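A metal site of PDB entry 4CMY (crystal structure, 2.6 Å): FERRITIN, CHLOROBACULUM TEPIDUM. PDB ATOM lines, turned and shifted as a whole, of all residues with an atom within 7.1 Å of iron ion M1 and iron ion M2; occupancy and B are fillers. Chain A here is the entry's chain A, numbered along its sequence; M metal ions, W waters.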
ATOM      1  N   GLN A  13      19.191   9.663 -17.489  1.00  0.00           N
ATOM      2  CA  GLN A  13      19.895   9.390 -16.255  1.00  0.00           C
ATOM      3  C   GLN A  13      21.358   9.790 -16.351  1.00  0.00           C
ATOM      4  O   GLN A  13      21.944  10.318 -15.414  1.00  0.00           O
ATOM      5  CB  GLN A  13      19.763   7.917 -15.927  1.00  0.00           C
ATOM      6  CG  GLN A  13      20.113   7.595 -14.480  1.00  0.00           C
ATOM      7  CD  GLN A  13      19.149   8.192 -13.509  1.00  0.00           C
ATOM      8  OE1 GLN A  13      17.959   8.308 -13.800  1.00  0.00           O
ATOM      9  NE2 GLN A  13      19.639   8.585 -12.348  1.00  0.00           N
ATOM     10  N   PHE A  16      21.294  13.323 -15.690  1.00  0.00           N
ATOM     11  CA  PHE A  16      20.946  13.557 -14.298  1.00  0.00           C
ATOM     12  C   PHE A  16      22.171  13.363 -13.379  1.00  0.00           C
ATOM     13  O   PHE A  16      22.434  14.171 -12.502  1.00  0.00           O
ATOM     14  CB  PHE A  16      19.814  12.591 -13.898  1.00  0.00           C
ATOM     15  CG  PHE A  16      18.935  13.053 -12.783  1.00  0.00           C
ATOM     16  CD1 PHE A  16      19.167  14.240 -12.076  1.00  0.00           C
ATOM     17  CD2 PHE A  16      17.888  12.254 -12.375  1.00  0.00           C
ATOM     18  CE1 PHE A  16      18.326  14.623 -11.039  1.00  0.00           C
ATOM     19  CE2 PHE A  16      17.075  12.628 -11.307  1.00  0.00           C
ATOM     20  CZ  PHE A  16      17.289  13.806 -10.661  1.00  0.00           C
ATOM     21  N   GLU A  17      22.939  12.312 -13.616  1.00  0.00           N
ATOM     22  CA  GLU A  17      24.157  12.079 -12.836  1.00  0.00           C
ATOM     23  C   GLU A  17      25.181  13.175 -13.097  1.00  0.00           C
ATOM     24  O   GLU A  17      25.802  13.691 -12.166  1.00  0.00           O
ATOM     25  CB  GLU A  17      24.752  10.691 -13.111  1.00  0.00           C
ATOM     26  CG  GLU A  17      23.804   9.537 -12.839  1.00  0.00           C
ATOM     27  CD  GLU A  17      23.495   9.270 -11.366  1.00  0.00           C
ATOM     28  OE1 GLU A  17      24.286   9.660 -10.443  1.00  0.00           O
ATOM     29  OE2 GLU A  17      22.471   8.538 -11.104  1.00  0.00           O
ATOM     30  N   SER A  20      24.221  16.112 -11.134  1.00  0.00           N
ATOM     31  CA  SER A  20      24.492  15.910  -9.716  1.00  0.00           C
ATOM     32  C   SER A  20      25.910  16.227  -9.363  1.00  0.00           C
ATOM     33  O   SER A  20      26.176  16.863  -8.386  1.00  0.00           O
ATOM     34  CB  SER A  20      24.197  14.462  -9.307  1.00  0.00           C
ATOM     35  OG  SER A  20      22.890  14.113  -9.700  1.00  0.00           O
ATOM     36  N   TYR A  24      26.872  19.187  -6.787  1.00  0.00           N
ATOM     37  CA  TYR A  24      27.685  18.993  -5.598  1.00  0.00           C
ATOM     38  C   TYR A  24      28.998  19.810  -5.621  1.00  0.00           C
ATOM     39  O   TYR A  24      29.471  20.263  -4.571  1.00  0.00           O
ATOM     40  CB  TYR A  24      27.930  17.521  -5.361  1.00  0.00           C
ATOM     41  CG  TYR A  24      26.674  16.722  -5.092  1.00  0.00           C
ATOM     42  CD1 TYR A  24      25.548  17.293  -4.548  1.00  0.00           C
ATOM     43  CD2 TYR A  24      26.630  15.364  -5.342  1.00  0.00           C
ATOM     44  CE1 TYR A  24      24.425  16.554  -4.283  1.00  0.00           C
ATOM     45  CE2 TYR A  24      25.518  14.629  -5.069  1.00  0.00           C
ATOM     46  CZ  TYR A  24      24.417  15.232  -4.527  1.00  0.00           C
ATOM     47  OH  TYR A  24      23.271  14.474  -4.257  1.00  0.00           O
ATOM     48  N   HIS A  46      32.198  13.799  -3.320  1.00  0.00           N
ATOM     49  CA  HIS A  46      31.015  13.127  -3.797  1.00  0.00           C
ATOM     50  C   HIS A  46      30.676  13.488  -5.227  1.00  0.00           C
ATOM     51  O   HIS A  46      30.008  12.721  -5.904  1.00  0.00           O
ATOM     52  CB  HIS A  46      29.821  13.371  -2.888  1.00  0.00           C
ATOM     53  CG  HIS A  46      28.894  12.228  -2.886  1.00  0.00           C
ATOM     54  ND1 HIS A  46      29.153  11.085  -2.156  1.00  0.00           N
ATOM     55  CD2 HIS A  46      27.792  11.969  -3.622  1.00  0.00           C
ATOM     56  CE1 HIS A  46      28.206  10.195  -2.403  1.00  0.00           C
ATOM     57  NE2 HIS A  46      27.375  10.713  -3.285  1.00  0.00           N
ATOM     58  N   GLU A  49      32.061  10.865  -7.167  1.00  0.00           N
ATOM     59  CA  GLU A  49      31.253   9.659  -7.161  1.00  0.00           C
ATOM     60  C   GLU A  49      30.145   9.748  -8.206  1.00  0.00           C
ATOM     61  O   GLU A  49      29.865   8.769  -8.887  1.00  0.00           O
ATOM     62  CB  GLU A  49      30.649   9.410  -5.777  1.00  0.00           C
ATOM     63  CG  GLU A  49      31.625   8.805  -4.786  1.00  0.00           C
ATOM     64  CD  GLU A  49      31.910   7.340  -5.091  1.00  0.00           C
ATOM     65  OE1 GLU A  49      30.973   6.537  -5.464  1.00  0.00           O
ATOM     66  OE2 GLU A  49      33.105   7.014  -5.007  1.00  0.00           O
ATOM     67  N   GLU A  50      29.519  10.900  -8.318  1.00  0.00           N
ATOM     68  CA  GLU A  50      28.445  11.078  -9.277  1.00  0.00           C
ATOM     69  C   GLU A  50      28.969  10.974 -10.694  1.00  0.00           C
ATOM     70  O   GLU A  50      28.301  10.462 -11.573  1.00  0.00           O
ATOM     71  CB  GLU A  50      27.686  12.400  -9.054  1.00  0.00           C
ATOM     72  CG  GLU A  50      27.017  12.477  -7.687  1.00  0.00           C
ATOM     73  CD  GLU A  50      25.891  11.452  -7.446  1.00  0.00           C
ATOM     74  OE1 GLU A  50      25.451  10.786  -8.429  1.00  0.00           O
ATOM     75  OE2 GLU A  50      25.436  11.335  -6.231  1.00  0.00           O
ATOM     76  N   LYS A  51      30.185  11.407 -10.917  1.00  0.00           N
ATOM     77  CA  LYS A  51      30.794  11.215 -12.202  1.00  0.00           C
ATOM     78  C   LYS A  51      31.016   9.798 -12.558  1.00  0.00           C
ATOM     79  O   LYS A  51      30.806   9.422 -13.692  1.00  0.00           O
ATOM     80  CB  LYS A  51      32.123  11.878 -12.192  1.00  0.00           C
ATOM     81  CG  LYS A  51      32.348  12.456 -13.501  1.00  0.00           C
ATOM     82  CD  LYS A  51      33.797  12.864 -13.710  1.00  0.00           C
ATOM     83  CE  LYS A  51      34.359  11.869 -14.668  1.00  0.00           C
ATOM     84  NZ  LYS A  51      35.530  12.330 -15.438  1.00  0.00           N
ATOM     85  N   HIS A  53      29.094   7.400 -11.499  1.00  0.00           N
ATOM     86  CA  HIS A  53      27.769   6.890 -11.792  1.00  0.00           C
ATOM     87  C   HIS A  53      27.423   7.210 -13.230  1.00  0.00           C
ATOM     88  O   HIS A  53      26.853   6.382 -13.938  1.00  0.00           O
ATOM     89  CB  HIS A  53      26.693   7.492 -10.908  1.00  0.00           C
ATOM     90  CG  HIS A  53      26.857   7.190  -9.450  1.00  0.00           C
ATOM     91  ND1 HIS A  53      26.115   7.834  -8.487  1.00  0.00           N
ATOM     92  CD2 HIS A  53      27.725   6.387  -8.796  1.00  0.00           C
ATOM     93  CE1 HIS A  53      26.496   7.402  -7.299  1.00  0.00           C
ATOM     94  NE2 HIS A  53      27.473   6.528  -7.453  1.00  0.00           N
ATOM     95  N   MET A  54      27.757   8.420 -13.646  1.00  0.00           N
ATOM     96  CA  MET A  54      27.497   8.859 -15.011  1.00  0.00           C
ATOM     97  C   MET A  54      28.235   7.975 -16.009  1.00  0.00           C
ATOM     98  O   MET A  54      27.616   7.499 -16.964  1.00  0.00           O
ATOM     99  CB  MET A  54      27.909  10.311 -15.188  1.00  0.00           C
ATOM    100  CG  MET A  54      27.733  10.811 -16.604  1.00  0.00           C
ATOM    101  SD  MET A  54      28.513  12.423 -16.852  1.00  0.00           S
ATOM    102  CE  MET A  54      30.189  11.888 -17.028  1.00  0.00           C
ATOM    103  N   HIS A  93      17.368  15.945  -3.719  1.00  0.00           N
ATOM    104  CA  HIS A  93      17.976  15.629  -5.001  1.00  0.00           C
ATOM    105  C   HIS A  93      18.305  14.129  -5.078  1.00  0.00           C
ATOM    106  O   HIS A  93      17.955  13.469  -6.051  1.00  0.00           O
ATOM    107  CB  HIS A  93      19.233  16.463  -5.184  1.00  0.00           C
ATOM    108  CG  HIS A  93      19.908  16.238  -6.470  1.00  0.00           C
ATOM    109  ND1 HIS A  93      19.536  16.903  -7.626  1.00  0.00           N
ATOM    110  CD2 HIS A  93      20.884  15.367  -6.831  1.00  0.00           C
ATOM    111  CE1 HIS A  93      20.280  16.469  -8.626  1.00  0.00           C
ATOM    112  NE2 HIS A  93      21.090  15.533  -8.180  1.00  0.00           N
ATOM    113  N   GLU A  94      18.871  13.575  -4.014  1.00  0.00           N
ATOM    114  CA  GLU A  94      19.090  12.137  -3.979  1.00  0.00           C
ATOM    115  C   GLU A  94      17.789  11.308  -4.019  1.00  0.00           C
ATOM    116  O   GLU A  94      17.757  10.260  -4.660  1.00  0.00           O
ATOM    117  CB  GLU A  94      20.003  11.727  -2.805  1.00  0.00           C
ATOM    118  CG  GLU A  94      21.463  12.140  -3.006  1.00  0.00           C
ATOM    119  CD  GLU A  94      22.207  11.315  -4.059  1.00  0.00           C
ATOM    120  OE1 GLU A  94      21.707  10.196  -4.349  1.00  0.00           O
ATOM    121  OE2 GLU A  94      23.318  11.751  -4.559  1.00  0.00           O
ATOM    122  N   ILE A  97      16.775  11.192  -7.571  1.00  0.00           N
ATOM    123  CA  ILE A  97      17.591  10.267  -8.335  1.00  0.00           C
ATOM    124  C   ILE A  97      17.051   8.879  -8.125  1.00  0.00           C
ATOM    125  O   ILE A  97      16.890   8.124  -9.062  1.00  0.00           O
ATOM    126  CB  ILE A  97      19.069  10.343  -7.954  1.00  0.00           C
ATOM    127  CG1 ILE A  97      19.677  11.634  -8.523  1.00  0.00           C
ATOM    128  CG2 ILE A  97      19.855   9.205  -8.561  1.00  0.00           C
ATOM    129  CD1 ILE A  97      20.994  11.989  -7.901  1.00  0.00           C
ATOM    130  N   ILE A 101      15.712   6.229 -10.918  1.00  0.00           N
ATOM    131  CA  ILE A 101      16.239   4.886 -11.067  1.00  0.00           C
ATOM    132  C   ILE A 101      15.109   3.874 -10.932  1.00  0.00           C
ATOM    133  O   ILE A 101      15.029   2.927 -11.728  1.00  0.00           O
ATOM    134  CB  ILE A 101      17.313   4.569 -10.022  1.00  0.00           C
ATOM    135  CG1 ILE A 101      18.574   5.411 -10.216  1.00  0.00           C
ATOM    136  CG2 ILE A 101      17.691   3.083 -10.060  1.00  0.00           C
ATOM    137  CD1 ILE A 101      19.330   5.137 -11.501  1.00  0.00           C
ATOM    138  N   TRP A 122      22.871  -2.512  -9.559  1.00  0.00           N
ATOM    139  CA  TRP A 122      23.974  -1.763  -8.955  1.00  0.00           C
ATOM    140  C   TRP A 122      23.487  -0.390  -8.451  1.00  0.00           C
ATOM    141  O   TRP A 122      23.795  -0.007  -7.322  1.00  0.00           O
ATOM    142  CB  TRP A 122      25.099  -1.580  -9.952  1.00  0.00           C
ATOM    143  CG  TRP A 122      26.288  -1.028  -9.343  1.00  0.00           C
ATOM    144  CD1 TRP A 122      27.262  -1.733  -8.749  1.00  0.00           C
ATOM    145  CD2 TRP A 122      26.631   0.360  -9.190  1.00  0.00           C
ATOM    146  NE1 TRP A 122      28.211  -0.869  -8.245  1.00  0.00           N
ATOM    147  CE2 TRP A 122      27.847   0.423  -8.513  1.00  0.00           C
ATOM    148  CE3 TRP A 122      26.031   1.560  -9.587  1.00  0.00           C
ATOM    149  CZ2 TRP A 122      28.495   1.604  -8.211  1.00  0.00           C
ATOM    150  CZ3 TRP A 122      26.681   2.747  -9.317  1.00  0.00           C
ATOM    151  CH2 TRP A 122      27.892   2.761  -8.606  1.00  0.00           C
ATOM    152  N   TYR A 123      22.707   0.334  -9.269  1.00  0.00           N
ATOM    153  CA  TYR A 123      22.197   1.671  -8.908  1.00  0.00           C
ATOM    154  C   TYR A 123      21.156   1.631  -7.810  1.00  0.00           C
ATOM    155  O   TYR A 123      21.107   2.518  -6.979  1.00  0.00           O
ATOM    156  CB  TYR A 123      21.618   2.414 -10.119  1.00  0.00           C
ATOM    157  CG  TYR A 123      22.679   2.859 -11.060  1.00  0.00           C
ATOM    158  CD1 TYR A 123      23.194   1.990 -11.990  1.00  0.00           C
ATOM    159  CD2 TYR A 123      23.234   4.122 -10.965  1.00  0.00           C
ATOM    160  CE1 TYR A 123      24.217   2.362 -12.824  1.00  0.00           C
ATOM    161  CE2 TYR A 123      24.260   4.503 -11.809  1.00  0.00           C
ATOM    162  CZ  TYR A 123      24.747   3.604 -12.747  1.00  0.00           C
ATOM    163  OH  TYR A 123      25.760   3.937 -13.597  1.00  0.00           O
ATOM    164  N   GLU A 126      23.217   1.240  -4.800  1.00  0.00           N
ATOM    165  CA  GLU A 126      23.969   2.448  -4.531  1.00  0.00           C
ATOM    166  C   GLU A 126      23.078   3.541  -3.983  1.00  0.00           C
ATOM    167  O   GLU A 126      23.480   4.280  -3.088  1.00  0.00           O
ATOM    168  CB  GLU A 126      24.704   2.918  -5.768  1.00  0.00           C
ATOM    169  CG  GLU A 126      25.773   4.012  -5.507  1.00  0.00           C
ATOM    170  CD  GLU A 126      27.053   3.534  -4.790  1.00  0.00           C
ATOM    171  OE1 GLU A 126      27.271   2.298  -4.627  1.00  0.00           O
ATOM    172  OE2 GLU A 126      27.857   4.447  -4.426  1.00  0.00           O
ATOM    173  N   GLN A 127      21.847   3.638  -4.450  1.00  0.00           N
ATOM    174  CA  GLN A 127      20.958   4.725  -3.992  1.00  0.00           C
ATOM    175  C   GLN A 127      20.467   4.505  -2.579  1.00  0.00           C
ATOM    176  O   GLN A 127      20.209   5.441  -1.875  1.00  0.00           O
ATOM    177  CB  GLN A 127      19.798   4.941  -4.963  1.00  0.00           C
ATOM    178  CG  GLN A 127      20.290   5.639  -6.204  1.00  0.00           C
ATOM    179  CD  GLN A 127      20.856   7.025  -5.919  1.00  0.00           C
ATOM    180  OE1 GLN A 127      21.956   7.384  -6.390  1.00  0.00           O
ATOM    181  NE2 GLN A 127      20.093   7.836  -5.171  1.00  0.00           N
ATOM    182  N   GLU A 130      23.272   5.975  -0.743  1.00  0.00           N
ATOM    183  CA  GLU A 130      23.245   7.444  -0.878  1.00  0.00           C
ATOM    184  C   GLU A 130      22.189   8.070   0.015  1.00  0.00           C
ATOM    185  O   GLU A 130      22.434   9.059   0.680  1.00  0.00           O
ATOM    186  CB  GLU A 130      22.919   7.853  -2.302  1.00  0.00           C
ATOM    187  CG  GLU A 130      23.940   7.487  -3.349  1.00  0.00           C
ATOM    188  CD  GLU A 130      25.062   8.490  -3.428  1.00  0.00           C
ATOM    189  OE1 GLU A 130      24.943   9.521  -4.185  1.00  0.00           O
ATOM    190  OE2 GLU A 130      26.061   8.237  -2.711  1.00  0.00           O
ATOM    191  N   GLU A 131      20.983   7.501   0.025  1.00  0.00           N
ATOM    192  CA  GLU A 131      19.939   8.028   0.889  1.00  0.00           C
ATOM    193  C   GLU A 131      20.302   7.902   2.368  1.00  0.00           C
ATOM    194  O   GLU A 131      20.020   8.805   3.150  1.00  0.00           O
ATOM    195  CB  GLU A 131      18.628   7.313   0.672  1.00  0.00           C
ATOM    196  CG  GLU A 131      17.936   7.786  -0.594  1.00  0.00           C
ATOM    197  CD  GLU A 131      16.642   7.040  -0.858  1.00  0.00           C
ATOM    198  OE1 GLU A 131      15.974   6.603   0.108  1.00  0.00           O
ATOM    199  OE2 GLU A 131      16.317   6.857  -2.031  1.00  0.00           O
ATOM    200  N   PHE A 134      23.040  10.767   3.010  1.00  0.00           N
ATOM    201  CA  PHE A 134      22.520  12.145   3.000  1.00  0.00           C
ATOM    202  C   PHE A 134      21.403  12.400   4.024  1.00  0.00           C
ATOM    203  O   PHE A 134      21.364  13.460   4.618  1.00  0.00           O
ATOM    204  CB  PHE A 134      22.031  12.536   1.613  1.00  0.00           C
ATOM    205  CG  PHE A 134      23.145  12.836   0.660  1.00  0.00           C
ATOM    206  CD1 PHE A 134      23.729  11.844  -0.096  1.00  0.00           C
ATOM    207  CD2 PHE A 134      23.656  14.096   0.573  1.00  0.00           C
ATOM    208  CE1 PHE A 134      24.773  12.111  -0.931  1.00  0.00           C
ATOM    209  CE2 PHE A 134      24.711  14.368  -0.254  1.00  0.00           C
ATOM    210  CZ  PHE A 134      25.264  13.377  -1.031  1.00  0.00           C
HETATM  211 FE    FE M   1      24.326   9.038  -8.532  1.00  0.00          FE
HETATM  212 FE    FE M   2      23.987  10.192  -5.707  1.00  0.00          FE
HETATM  213  O   HOH W   1      23.159   7.268  -9.107  1.00  0.00           O
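The side-chain carboxylate (OE2) of Glu 130 lies within hydrogen-bond range of a ring nitrogen (NE2) of His 46.
OE2 of Glu 17 sits at hydrogen-bond distance from NE2 of Gln 13, at 3.1 Å.
OE1 of Glu 94 lies within hydrogen-bond range of NE2 of Gln 127, 3.0 Å away.
The side-chain hydroxyl (OH) of Tyr 24 sits close to the side-chain carboxylate (OE2) of Glu 94 (2.7 Å).
The side-chain hydroxyl (OH) of Tyr 123 lies within hydrogen-bond range of the backbone carbonyl oxygen (O) of His 53, at 2.7 Å.
Merely in contact with iron ion M1: Gln 127.
Of the 22 residues printed, 4 come within 4 Å of iron ion M1.
OE1 of Gln 127 touches iron ion M2 (3.5 Å).
Within 4 Å of iron ion M2: Glu 50, Glu 94, Gln 127 and Glu 130.
The nearest printed residue that does not touch iron ion M2 is His 53 (4.1 Å).
The side-chain carboxylate (OE1) of Glu 17 binds iron ion M1.
OE1 of Glu 50 binds iron ion M1.
A ring nitrogen (ND1) of His 53 binds iron ion M1, at 2.2 Å.
Iron ion M1 is bound by water W1 (2.2 Å).
Iron ion M1 has four donor atoms within binding distance.
Iron ion M2 is bound by the side-chain carboxylate of Glu 50 (1.9 Å), the side-chain carboxylate of Glu 130 (1.9 Å) and the side-chain carboxylate of Glu 94 (2.0 Å).
Iron ion M2 has three donor atoms within binding distance.
Slightly farther from iron ion M2 lies the side-chain carboxylate (OE1) of Glu 94 (2.7 Å).
Water W1 bridges OE2 of Glu 17 (2.5 Å) and OE1 of Gln 127 (3.0 Å).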
